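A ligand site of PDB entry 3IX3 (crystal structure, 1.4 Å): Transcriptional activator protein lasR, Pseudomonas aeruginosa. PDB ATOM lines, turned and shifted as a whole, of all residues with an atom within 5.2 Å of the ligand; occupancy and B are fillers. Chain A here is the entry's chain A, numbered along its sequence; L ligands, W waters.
Water W1 lies within hydrogen-bond range of O1 of the ligand (2.8 Å) and NE of Arg 61 (3.0 Å).
OG of Ser 129 sits at hydrogen-bond distance from O2 of the ligand (2.7 Å).
The side-chain hydroxyl (OH) of Tyr 56 sits at hydrogen-bond distance from an oxygen (O2) of the ligand.
OD2 of Asp 73 is in hydrogen-bond range of N1 of the ligand (2.8 Å).
The indole nitrogen of Trp 60 is in hydrogen-bond range of an oxygen (O3) of the ligand (3.0 Å).
The side-chain hydroxyl (OG1) of Thr 75 lies close to a nitrogen (N1) of the ligand (3.5 Å).
The backbone NH of Ser 129 is in hydrogen-bond range of the backbone carbonyl oxygen of Leu 36 (2.8 Å).
The side-chain hydroxyl of Ser 129 lies within hydrogen-bond range of the side-chain hydroxyl of Thr 115 (2.8 Å).
OG1 of Thr 75 is in hydrogen-bond range of OD1 of Asp 73, at 2.8 Å.
The side-chain hydroxyl (OH) of Tyr 64 sits at hydrogen-bond distance from the side-chain carboxylate (OD2) of Asp 73 (2.7 Å).
The backbone carbonyl oxygen (O) of Thr 75 sits at hydrogen-bond distance from the side-chain sulfur (SG) of Cys 79 (3.3 Å).
SG of Cys 79 lies within hydrogen-bond range of O of Gly 126 (3.8 Å).
The indole nitrogen (NE1) of Trp 88 is in hydrogen-bond range of the side-chain hydroxyl (OG1) of Thr 115, at 2.9 Å.
The backbone NH of Gly 38 is in hydrogen-bond range of the backbone carbonyl oxygen of Ala 127.
Residues that only touch the ligand: Leu 36 (3.8 Å), Gly 38 (3.96 Å), Ala 50 (3.7 Å), Ile 52 (3.95 Å), Arg 61 (3.9 Å), Tyr 64 (3.4 Å), Val 76 (3.96 Å), Cys 79 (3.8 Å), Trp 88 (3.8 Å), Tyr 93 (3.4 Å), Phe 101 (3.9 Å), Ala 105 (3.3 Å), Leu 110 (3.6 Å) and Gly 126 (3.8 Å).
Of the 26 residues printed, 19 come within 4 Å of the ligand.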
ATOM      1  N   LEU A  36     -27.270 -21.991 -10.120  1.00  0.00           N
ATOM      2  CA  LEU A  36     -28.094 -20.890 -10.564  1.00  0.00           C
ATOM      3  C   LEU A  36     -28.265 -21.002 -12.068  1.00  0.00           C
ATOM      4  O   LEU A  36     -27.300 -21.118 -12.817  1.00  0.00           O
ATOM      5  CB  LEU A  36     -27.444 -19.544 -10.211  1.00  0.00           C
ATOM      6  CG  LEU A  36     -28.198 -18.288 -10.682  1.00  0.00           C
ATOM      7  CD1 LEU A  36     -28.135 -17.184  -9.641  1.00  0.00           C
ATOM      8  CD2 LEU A  36     -27.678 -17.806 -12.048  1.00  0.00           C
ATOM      9  N   GLY A  38     -29.879 -18.645 -14.947  1.00  0.00           N
ATOM     10  CA  GLY A  38     -30.376 -17.283 -15.149  1.00  0.00           C
ATOM     11  C   GLY A  38     -30.596 -17.066 -16.627  1.00  0.00           C
ATOM     12  O   GLY A  38     -29.786 -17.504 -17.446  1.00  0.00           O
ATOM     13  N   LEU A  39     -31.673 -16.366 -16.989  1.00  0.00           N
ATOM     14  CA  LEU A  39     -32.001 -16.209 -18.397  1.00  0.00           C
ATOM     15  C   LEU A  39     -32.720 -14.904 -18.637  1.00  0.00           C
ATOM     16  O   LEU A  39     -33.602 -14.506 -17.859  1.00  0.00           O
ATOM     17  CB  LEU A  39     -32.844 -17.399 -18.885  1.00  0.00           C
ATOM     18  CG  LEU A  39     -32.888 -17.646 -20.391  1.00  0.00           C
ATOM     19  CD1 LEU A  39     -31.565 -18.121 -20.927  1.00  0.00           C
ATOM     20  CD2 LEU A  39     -33.939 -18.677 -20.716  1.00  0.00           C
ATOM     21  N   LEU A  40     -32.334 -14.257 -19.750  1.00  0.00           N
ATOM     22  CA  LEU A  40     -32.951 -13.026 -20.219  1.00  0.00           C
ATOM     23  C   LEU A  40     -33.414 -13.212 -21.664  1.00  0.00           C
ATOM     24  O   LEU A  40     -32.800 -13.964 -22.439  1.00  0.00           O
ATOM     25  CB  LEU A  40     -31.929 -11.893 -20.207  1.00  0.00           C
ATOM     26  CG  LEU A  40     -31.649 -11.333 -18.816  1.00  0.00           C
ATOM     27  CD1 LEU A  40     -30.334 -10.574 -18.764  1.00  0.00           C
ATOM     28  CD2 LEU A  40     -32.806 -10.453 -18.332  1.00  0.00           C
ATOM     29  N   TYR A  47     -30.311  -7.316 -15.745  1.00  0.00           N
ATOM     30  CA  TYR A  47     -29.870  -8.484 -14.984  1.00  0.00           C
ATOM     31  C   TYR A  47     -30.648  -8.685 -13.692  1.00  0.00           C
ATOM     32  O   TYR A  47     -30.864  -9.807 -13.258  1.00  0.00           O
ATOM     33  CB  TYR A  47     -28.372  -8.401 -14.688  1.00  0.00           C
ATOM     34  CG  TYR A  47     -27.496  -8.292 -15.914  1.00  0.00           C
ATOM     35  CD1 TYR A  47     -26.635  -7.213 -16.070  1.00  0.00           C
ATOM     36  CD2 TYR A  47     -27.543  -9.255 -16.934  1.00  0.00           C
ATOM     37  CE1 TYR A  47     -25.809  -7.114 -17.195  1.00  0.00           C
ATOM     38  CE2 TYR A  47     -26.733  -9.155 -18.054  1.00  0.00           C
ATOM     39  CZ  TYR A  47     -25.883  -8.070 -18.182  1.00  0.00           C
ATOM     40  OH  TYR A  47     -25.081  -7.950 -19.308  1.00  0.00           O
ATOM     41  N   ALA A  50     -33.841 -10.791 -14.453  1.00  0.00           N
ATOM     42  CA  ALA A  50     -33.738 -12.066 -15.150  1.00  0.00           C
ATOM     43  C   ALA A  50     -34.650 -13.116 -14.531  1.00  0.00           C
ATOM     44  O   ALA A  50     -35.053 -13.056 -13.348  1.00  0.00           O
ATOM     45  CB  ALA A  50     -32.332 -12.548 -15.101  1.00  0.00           C
ATOM     46  N   ILE A  52     -34.653 -16.420 -12.830  1.00  0.00           N
ATOM     47  CA  ILE A  52     -33.648 -17.075 -11.995  1.00  0.00           C
ATOM     48  C   ILE A  52     -34.221 -18.338 -11.361  1.00  0.00           C
ATOM     49  O   ILE A  52     -35.297 -18.310 -10.744  1.00  0.00           O
ATOM     50  CB  ILE A  52     -33.163 -16.146 -10.840  1.00  0.00           C
ATOM     51  CG1 ILE A  52     -32.572 -14.833 -11.369  1.00  0.00           C
ATOM     52  CG2 ILE A  52     -32.140 -16.877  -9.951  1.00  0.00           C
ATOM     53  CD1 ILE A  52     -31.267 -14.968 -12.075  1.00  0.00           C
ATOM     54  N   TYR A  56     -28.839 -20.971  -4.808  1.00  0.00           N
ATOM     55  CA  TYR A  56     -27.913 -20.045  -4.141  1.00  0.00           C
ATOM     56  C   TYR A  56     -28.555 -19.518  -2.834  1.00  0.00           C
ATOM     57  O   TYR A  56     -29.800 -19.360  -2.760  1.00  0.00           O
ATOM     58  CB  TYR A  56     -27.577 -18.862  -5.063  1.00  0.00           C
ATOM     59  CG  TYR A  56     -26.474 -19.066  -6.079  1.00  0.00           C
ATOM     60  CD1 TYR A  56     -25.893 -17.980  -6.730  1.00  0.00           C
ATOM     61  CD2 TYR A  56     -26.011 -20.336  -6.407  1.00  0.00           C
ATOM     62  CE1 TYR A  56     -24.870 -18.138  -7.655  1.00  0.00           C
ATOM     63  CE2 TYR A  56     -25.001 -20.520  -7.353  1.00  0.00           C
ATOM     64  CZ  TYR A  56     -24.447 -19.428  -7.971  1.00  0.00           C
ATOM     65  OH  TYR A  56     -23.423 -19.644  -8.863  1.00  0.00           O
ATOM     66  N   TRP A  60     -27.609 -14.090  -0.369  1.00  0.00           N
ATOM     67  CA  TRP A  60     -26.625 -13.755  -1.384  1.00  0.00           C
ATOM     68  C   TRP A  60     -27.299 -13.239  -2.655  1.00  0.00           C
ATOM     69  O   TRP A  60     -26.867 -12.236  -3.202  1.00  0.00           O
ATOM     70  CB  TRP A  60     -25.760 -14.985  -1.712  1.00  0.00           C
ATOM     71  CG  TRP A  60     -24.800 -14.759  -2.866  1.00  0.00           C
ATOM     72  CD1 TRP A  60     -24.794 -15.430  -4.054  1.00  0.00           C
ATOM     73  CD2 TRP A  60     -23.727 -13.793  -2.932  1.00  0.00           C
ATOM     74  NE1 TRP A  60     -23.788 -14.939  -4.875  1.00  0.00           N
ATOM     75  CE2 TRP A  60     -23.124 -13.947  -4.208  1.00  0.00           C
ATOM     76  CE3 TRP A  60     -23.233 -12.813  -2.055  1.00  0.00           C
ATOM     77  CZ2 TRP A  60     -22.043 -13.159  -4.615  1.00  0.00           C
ATOM     78  CZ3 TRP A  60     -22.158 -12.033  -2.463  1.00  0.00           C
ATOM     79  CH2 TRP A  60     -21.578 -12.208  -3.732  1.00  0.00           C
ATOM     80  N   ARG A  61     -28.324 -13.943  -3.143  1.00  0.00           N
ATOM     81  CA  ARG A  61     -29.071 -13.470  -4.302  1.00  0.00           C
ATOM     82  C   ARG A  61     -29.574 -12.035  -4.076  1.00  0.00           C
ATOM     83  O   ARG A  61     -29.477 -11.182  -4.956  1.00  0.00           O
ATOM     84  CB  ARG A  61     -30.254 -14.408  -4.574  1.00  0.00           C
ATOM     85  CG  ARG A  61     -29.822 -15.761  -5.200  1.00  0.00           C
ATOM     86  CD  ARG A  61     -29.986 -15.784  -6.729  1.00  0.00           C
ATOM     87  NE  ARG A  61     -29.136 -14.795  -7.391  1.00  0.00           N
ATOM     88  CZ  ARG A  61     -29.550 -13.639  -7.902  1.00  0.00           C
ATOM     89  NH1 ARG A  61     -30.840 -13.286  -7.926  1.00  0.00           N
ATOM     90  NH2 ARG A  61     -28.666 -12.837  -8.460  1.00  0.00           N
ATOM     91  N   TYR A  64     -26.614  -9.603  -4.051  1.00  0.00           N
ATOM     92  CA  TYR A  64     -26.070  -9.541  -5.391  1.00  0.00           C
ATOM     93  C   TYR A  64     -26.879  -8.597  -6.286  1.00  0.00           C
ATOM     94  O   TYR A  64     -26.309  -7.735  -6.972  1.00  0.00           O
ATOM     95  CB  TYR A  64     -26.043 -10.966  -5.935  1.00  0.00           C
ATOM     96  CG  TYR A  64     -25.385 -11.185  -7.285  1.00  0.00           C
ATOM     97  CD1 TYR A  64     -24.174 -11.879  -7.397  1.00  0.00           C
ATOM     98  CD2 TYR A  64     -26.000 -10.771  -8.460  1.00  0.00           C
ATOM     99  CE1 TYR A  64     -23.582 -12.106  -8.640  1.00  0.00           C
ATOM    100  CE2 TYR A  64     -25.422 -10.988  -9.689  1.00  0.00           C
ATOM    101  CZ  TYR A  64     -24.205 -11.649  -9.783  1.00  0.00           C
ATOM    102  OH  TYR A  64     -23.650 -11.885 -11.028  1.00  0.00           O
ATOM    103  N   ALA A  70     -24.133  -8.050 -11.007  1.00  0.00           N
ATOM    104  CA  ALA A  70     -24.093  -8.611 -12.367  1.00  0.00           C
ATOM    105  C   ALA A  70     -23.161  -7.822 -13.274  1.00  0.00           C
ATOM    106  O   ALA A  70     -22.642  -8.360 -14.266  1.00  0.00           O
ATOM    107  CB  ALA A  70     -25.454  -8.694 -12.992  1.00  0.00           C
ATOM    108  N   ASP A  73     -19.377  -8.970 -11.622  1.00  0.00           N
ATOM    109  CA  ASP A  73     -19.085 -10.390 -11.679  1.00  0.00           C
ATOM    110  C   ASP A  73     -18.510 -10.760 -13.053  1.00  0.00           C
ATOM    111  O   ASP A  73     -19.178 -10.623 -14.062  1.00  0.00           O
ATOM    112  CB  ASP A  73     -20.415 -11.103 -11.443  1.00  0.00           C
ATOM    113  CG  ASP A  73     -20.300 -12.610 -11.375  1.00  0.00           C
ATOM    114  OD1 ASP A  73     -19.265 -13.175 -11.750  1.00  0.00           O
ATOM    115  OD2 ASP A  73     -21.313 -13.206 -10.958  1.00  0.00           O
ATOM    116  N   THR A  75     -18.094 -13.528 -14.446  1.00  0.00           N
ATOM    117  CA  THR A  75     -18.782 -14.628 -15.144  1.00  0.00           C
ATOM    118  C   THR A  75     -19.905 -14.089 -16.042  1.00  0.00           C
ATOM    119  O   THR A  75     -20.172 -14.661 -17.101  1.00  0.00           O
ATOM    120  CB  THR A  75     -19.311 -15.704 -14.172  1.00  0.00           C
ATOM    121  OG1 THR A  75     -20.373 -15.168 -13.368  1.00  0.00           O
ATOM    122  CG2 THR A  75     -18.221 -16.278 -13.301  1.00  0.00           C
ATOM    123  N   VAL A  76     -20.516 -12.991 -15.649  1.00  0.00           N
ATOM    124  CA  VAL A  76     -21.612 -12.435 -16.433  1.00  0.00           C
ATOM    125  C   VAL A  76     -21.076 -11.805 -17.714  1.00  0.00           C
ATOM    126  O   VAL A  76     -21.577 -12.079 -18.809  1.00  0.00           O
ATOM    127  CB  VAL A  76     -22.450 -11.417 -15.630  1.00  0.00           C
ATOM    128  CG1 VAL A  76     -23.472 -10.739 -16.530  1.00  0.00           C
ATOM    129  CG2 VAL A  76     -23.140 -12.162 -14.502  1.00  0.00           C
ATOM    130  N   CYS A  79     -20.208 -14.434 -20.204  1.00  0.00           N
ATOM    131  CA  CYS A  79     -21.367 -14.998 -20.909  1.00  0.00           C
ATOM    132  C   CYS A  79     -21.813 -14.147 -22.086  1.00  0.00           C
ATOM    133  O   CYS A  79     -22.321 -14.680 -23.068  1.00  0.00           O
ATOM    134  CB  CYS A  79     -22.561 -15.185 -19.957  1.00  0.00           C
ATOM    135  SG  CYS A  79     -22.330 -16.491 -18.748  1.00  0.00           S
ATOM    136  N   TRP A  88     -14.276 -20.793 -12.064  1.00  0.00           N
ATOM    137  CA  TRP A  88     -14.072 -19.797 -11.004  1.00  0.00           C
ATOM    138  C   TRP A  88     -12.738 -19.990 -10.313  1.00  0.00           C
ATOM    139  O   TRP A  88     -12.446 -21.034  -9.740  1.00  0.00           O
ATOM    140  CB  TRP A  88     -15.152 -19.895  -9.952  1.00  0.00           C
ATOM    141  CG  TRP A  88     -16.586 -19.855 -10.423  1.00  0.00           C
ATOM    142  CD1 TRP A  88     -17.055 -19.530 -11.667  1.00  0.00           C
ATOM    143  CD2 TRP A  88     -17.710 -20.150  -9.619  1.00  0.00           C
ATOM    144  NE1 TRP A  88     -18.443 -19.623 -11.672  1.00  0.00           N
ATOM    145  CE2 TRP A  88     -18.860 -19.997 -10.419  1.00  0.00           C
ATOM    146  CE3 TRP A  88     -17.863 -20.548  -8.275  1.00  0.00           C
ATOM    147  CZ2 TRP A  88     -20.152 -20.230  -9.928  1.00  0.00           C
ATOM    148  CZ3 TRP A  88     -19.145 -20.776  -7.791  1.00  0.00           C
ATOM    149  CH2 TRP A  88     -20.272 -20.613  -8.617  1.00  0.00           C
ATOM    150  N   TYR A  93     -10.856 -12.654 -11.315  1.00  0.00           N
ATOM    151  CA  TYR A  93     -11.238 -11.463 -10.573  1.00  0.00           C
ATOM    152  C   TYR A  93     -10.064 -10.497 -10.689  1.00  0.00           C
ATOM    153  O   TYR A  93      -9.069 -10.617  -9.953  1.00  0.00           O
ATOM    154  CB  TYR A  93     -11.554 -11.838  -9.131  1.00  0.00           C
ATOM    155  CG  TYR A  93     -12.666 -12.855  -9.026  1.00  0.00           C
ATOM    156  CD1 TYR A  93     -12.377 -14.184  -8.712  1.00  0.00           C
ATOM    157  CD2 TYR A  93     -13.992 -12.503  -9.226  1.00  0.00           C
ATOM    158  CE1 TYR A  93     -13.393 -15.136  -8.617  1.00  0.00           C
ATOM    159  CE2 TYR A  93     -15.002 -13.433  -9.133  1.00  0.00           C
ATOM    160  CZ  TYR A  93     -14.713 -14.748  -8.821  1.00  0.00           C
ATOM    161  OH  TYR A  93     -15.758 -15.636  -8.728  1.00  0.00           O
ATOM    162  N   PHE A 101     -15.841  -8.202  -4.815  1.00  0.00           N
ATOM    163  CA  PHE A 101     -16.887  -9.173  -5.128  1.00  0.00           C
ATOM    164  C   PHE A 101     -16.472 -10.589  -4.761  1.00  0.00           C
ATOM    165  O   PHE A 101     -17.231 -11.322  -4.127  1.00  0.00           O
ATOM    166  CB  PHE A 101     -17.256  -9.077  -6.616  1.00  0.00           C
ATOM    167  CG  PHE A 101     -18.154 -10.197  -7.073  1.00  0.00           C
ATOM    168  CD1 PHE A 101     -19.516 -10.160  -6.801  1.00  0.00           C
ATOM    169  CD2 PHE A 101     -17.639 -11.299  -7.749  1.00  0.00           C
ATOM    170  CE1 PHE A 101     -20.337 -11.195  -7.202  1.00  0.00           C
ATOM    171  CE2 PHE A 101     -18.459 -12.334  -8.151  1.00  0.00           C
ATOM    172  CZ  PHE A 101     -19.808 -12.295  -7.875  1.00  0.00           C
ATOM    173  N   ALA A 105     -18.363 -13.277  -2.436  1.00  0.00           N
ATOM    174  CA  ALA A 105     -18.820 -14.537  -2.995  1.00  0.00           C
ATOM    175  C   ALA A 105     -18.216 -15.700  -2.229  1.00  0.00           C
ATOM    176  O   ALA A 105     -18.892 -16.689  -1.936  1.00  0.00           O
ATOM    177  CB  ALA A 105     -18.456 -14.609  -4.472  1.00  0.00           C
ATOM    178  N   LEU A 110     -19.195 -19.584  -2.420  1.00  0.00           N
ATOM    179  CA  LEU A 110     -19.131 -19.772  -3.866  1.00  0.00           C
ATOM    180  C   LEU A 110     -17.686 -19.654  -4.376  1.00  0.00           C
ATOM    181  O   LEU A 110     -17.292 -18.686  -5.018  1.00  0.00           O
ATOM    182  CB  LEU A 110     -20.091 -18.814  -4.571  1.00  0.00           C
ATOM    183  CG  LEU A 110     -21.574 -19.100  -4.270  1.00  0.00           C
ATOM    184  CD1 LEU A 110     -22.463 -17.956  -4.713  1.00  0.00           C
ATOM    185  CD2 LEU A 110     -22.025 -20.367  -4.933  1.00  0.00           C
ATOM    186  N   THR A 115     -19.185 -21.486 -14.699  1.00  0.00           N
ATOM    187  CA  THR A 115     -20.388 -20.948 -15.345  1.00  0.00           C
ATOM    188  C   THR A 115     -20.380 -21.282 -16.826  1.00  0.00           C
ATOM    189  O   THR A 115     -19.384 -21.034 -17.527  1.00  0.00           O
ATOM    190  CB  THR A 115     -20.466 -19.423 -15.155  1.00  0.00           C
ATOM    191  OG1 THR A 115     -20.482 -19.140 -13.743  1.00  0.00           O
ATOM    192  CG2 THR A 115     -21.710 -18.820 -15.829  1.00  0.00           C
ATOM    193  N   LEU A 125     -30.233 -14.918 -23.560  1.00  0.00           N
ATOM    194  CA  LEU A 125     -28.893 -14.828 -22.965  1.00  0.00           C
ATOM    195  C   LEU A 125     -28.989 -15.337 -21.535  1.00  0.00           C
ATOM    196  O   LEU A 125     -29.855 -14.897 -20.770  1.00  0.00           O
ATOM    197  CB  LEU A 125     -28.386 -13.377 -22.924  1.00  0.00           C
ATOM    198  CG  LEU A 125     -27.157 -13.120 -22.034  1.00  0.00           C
ATOM    199  CD1 LEU A 125     -25.900 -13.744 -22.619  1.00  0.00           C
ATOM    200  CD2 LEU A 125     -26.968 -11.622 -21.869  1.00  0.00           C
ATOM    201  N   GLY A 126     -28.107 -16.242 -21.162  1.00  0.00           N
ATOM    202  CA  GLY A 126     -28.153 -16.759 -19.809  1.00  0.00           C
ATOM    203  C   GLY A 126     -26.863 -17.343 -19.295  1.00  0.00           C
ATOM    204  O   GLY A 126     -25.799 -17.278 -19.946  1.00  0.00           O
ATOM    205  N   ALA A 127     -26.989 -17.967 -18.135  1.00  0.00           N
ATOM    206  CA  ALA A 127     -25.881 -18.614 -17.448  1.00  0.00           C
ATOM    207  C   ALA A 127     -26.392 -19.813 -16.685  1.00  0.00           C
ATOM    208  O   ALA A 127     -27.439 -19.736 -16.012  1.00  0.00           O
ATOM    209  CB  ALA A 127     -25.240 -17.653 -16.469  1.00  0.00           C
ATOM    210  N   SER A 129     -24.714 -21.680 -13.716  1.00  0.00           N
ATOM    211  CA  SER A 129     -23.607 -21.734 -12.778  1.00  0.00           C
ATOM    212  C   SER A 129     -23.743 -22.903 -11.850  1.00  0.00           C
ATOM    213  O   SER A 129     -24.843 -23.207 -11.371  1.00  0.00           O
ATOM    214  CB  SER A 129     -23.567 -20.465 -11.951  1.00  0.00           C
ATOM    215  OG  SER A 129     -23.109 -19.389 -12.742  1.00  0.00           O
HETATM  216  C1  LIG L   1     -25.645 -13.840 -18.280  1.00  0.00           C
HETATM  217  C2  LIG L   1     -26.850 -13.161 -17.644  1.00  0.00           C
HETATM  218  C3  LIG L   1     -27.791 -14.119 -16.924  1.00  0.00           C
HETATM  219  C4  LIG L   1     -28.911 -13.394 -16.178  1.00  0.00           C
HETATM  220  C5  LIG L   1     -28.476 -12.633 -14.922  1.00  0.00           C
HETATM  221  C6  LIG L   1     -28.015 -13.651 -13.891  1.00  0.00           C
HETATM  222  C7  LIG L   1     -27.555 -12.966 -12.620  1.00  0.00           C
HETATM  223  C8  LIG L   1     -26.799 -13.921 -11.699  1.00  0.00           C
HETATM  224  C9  LIG L   1     -25.510 -14.474 -12.330  1.00  0.00           C
HETATM  225  C10 LIG L   1     -24.588 -15.153 -11.358  1.00  0.00           C
HETATM  226  O1  LIG L   1     -24.871 -15.263 -10.172  1.00  0.00           O
HETATM  227  C11 LIG L   1     -23.287 -15.660 -11.906  1.00  0.00           C
HETATM  228  C12 LIG L   1     -22.581 -16.492 -10.876  1.00  0.00           C
HETATM  229  O2  LIG L   1     -22.929 -17.658 -10.676  1.00  0.00           O
HETATM  230  N1  LIG L   1     -21.604 -15.886 -10.223  1.00  0.00           N
HETATM  231  C13 LIG L   1     -20.882 -16.576  -9.172  1.00  0.00           C
HETATM  232  C14 LIG L   1     -19.359 -16.392  -9.232  1.00  0.00           C
HETATM  233  C15 LIG L   1     -18.922 -16.529  -7.777  1.00  0.00           C
HETATM  234  C16 LIG L   1     -21.179 -16.004  -7.833  1.00  0.00           C
HETATM  235  O3  LIG L   1     -22.237 -15.583  -7.417  1.00  0.00           O
HETATM  236  O4  LIG L   1     -20.028 -16.067  -7.018  1.00  0.00           O
HETATM  237  O   HOH W   1     -26.201 -14.507  -7.820  1.00  0.00           O
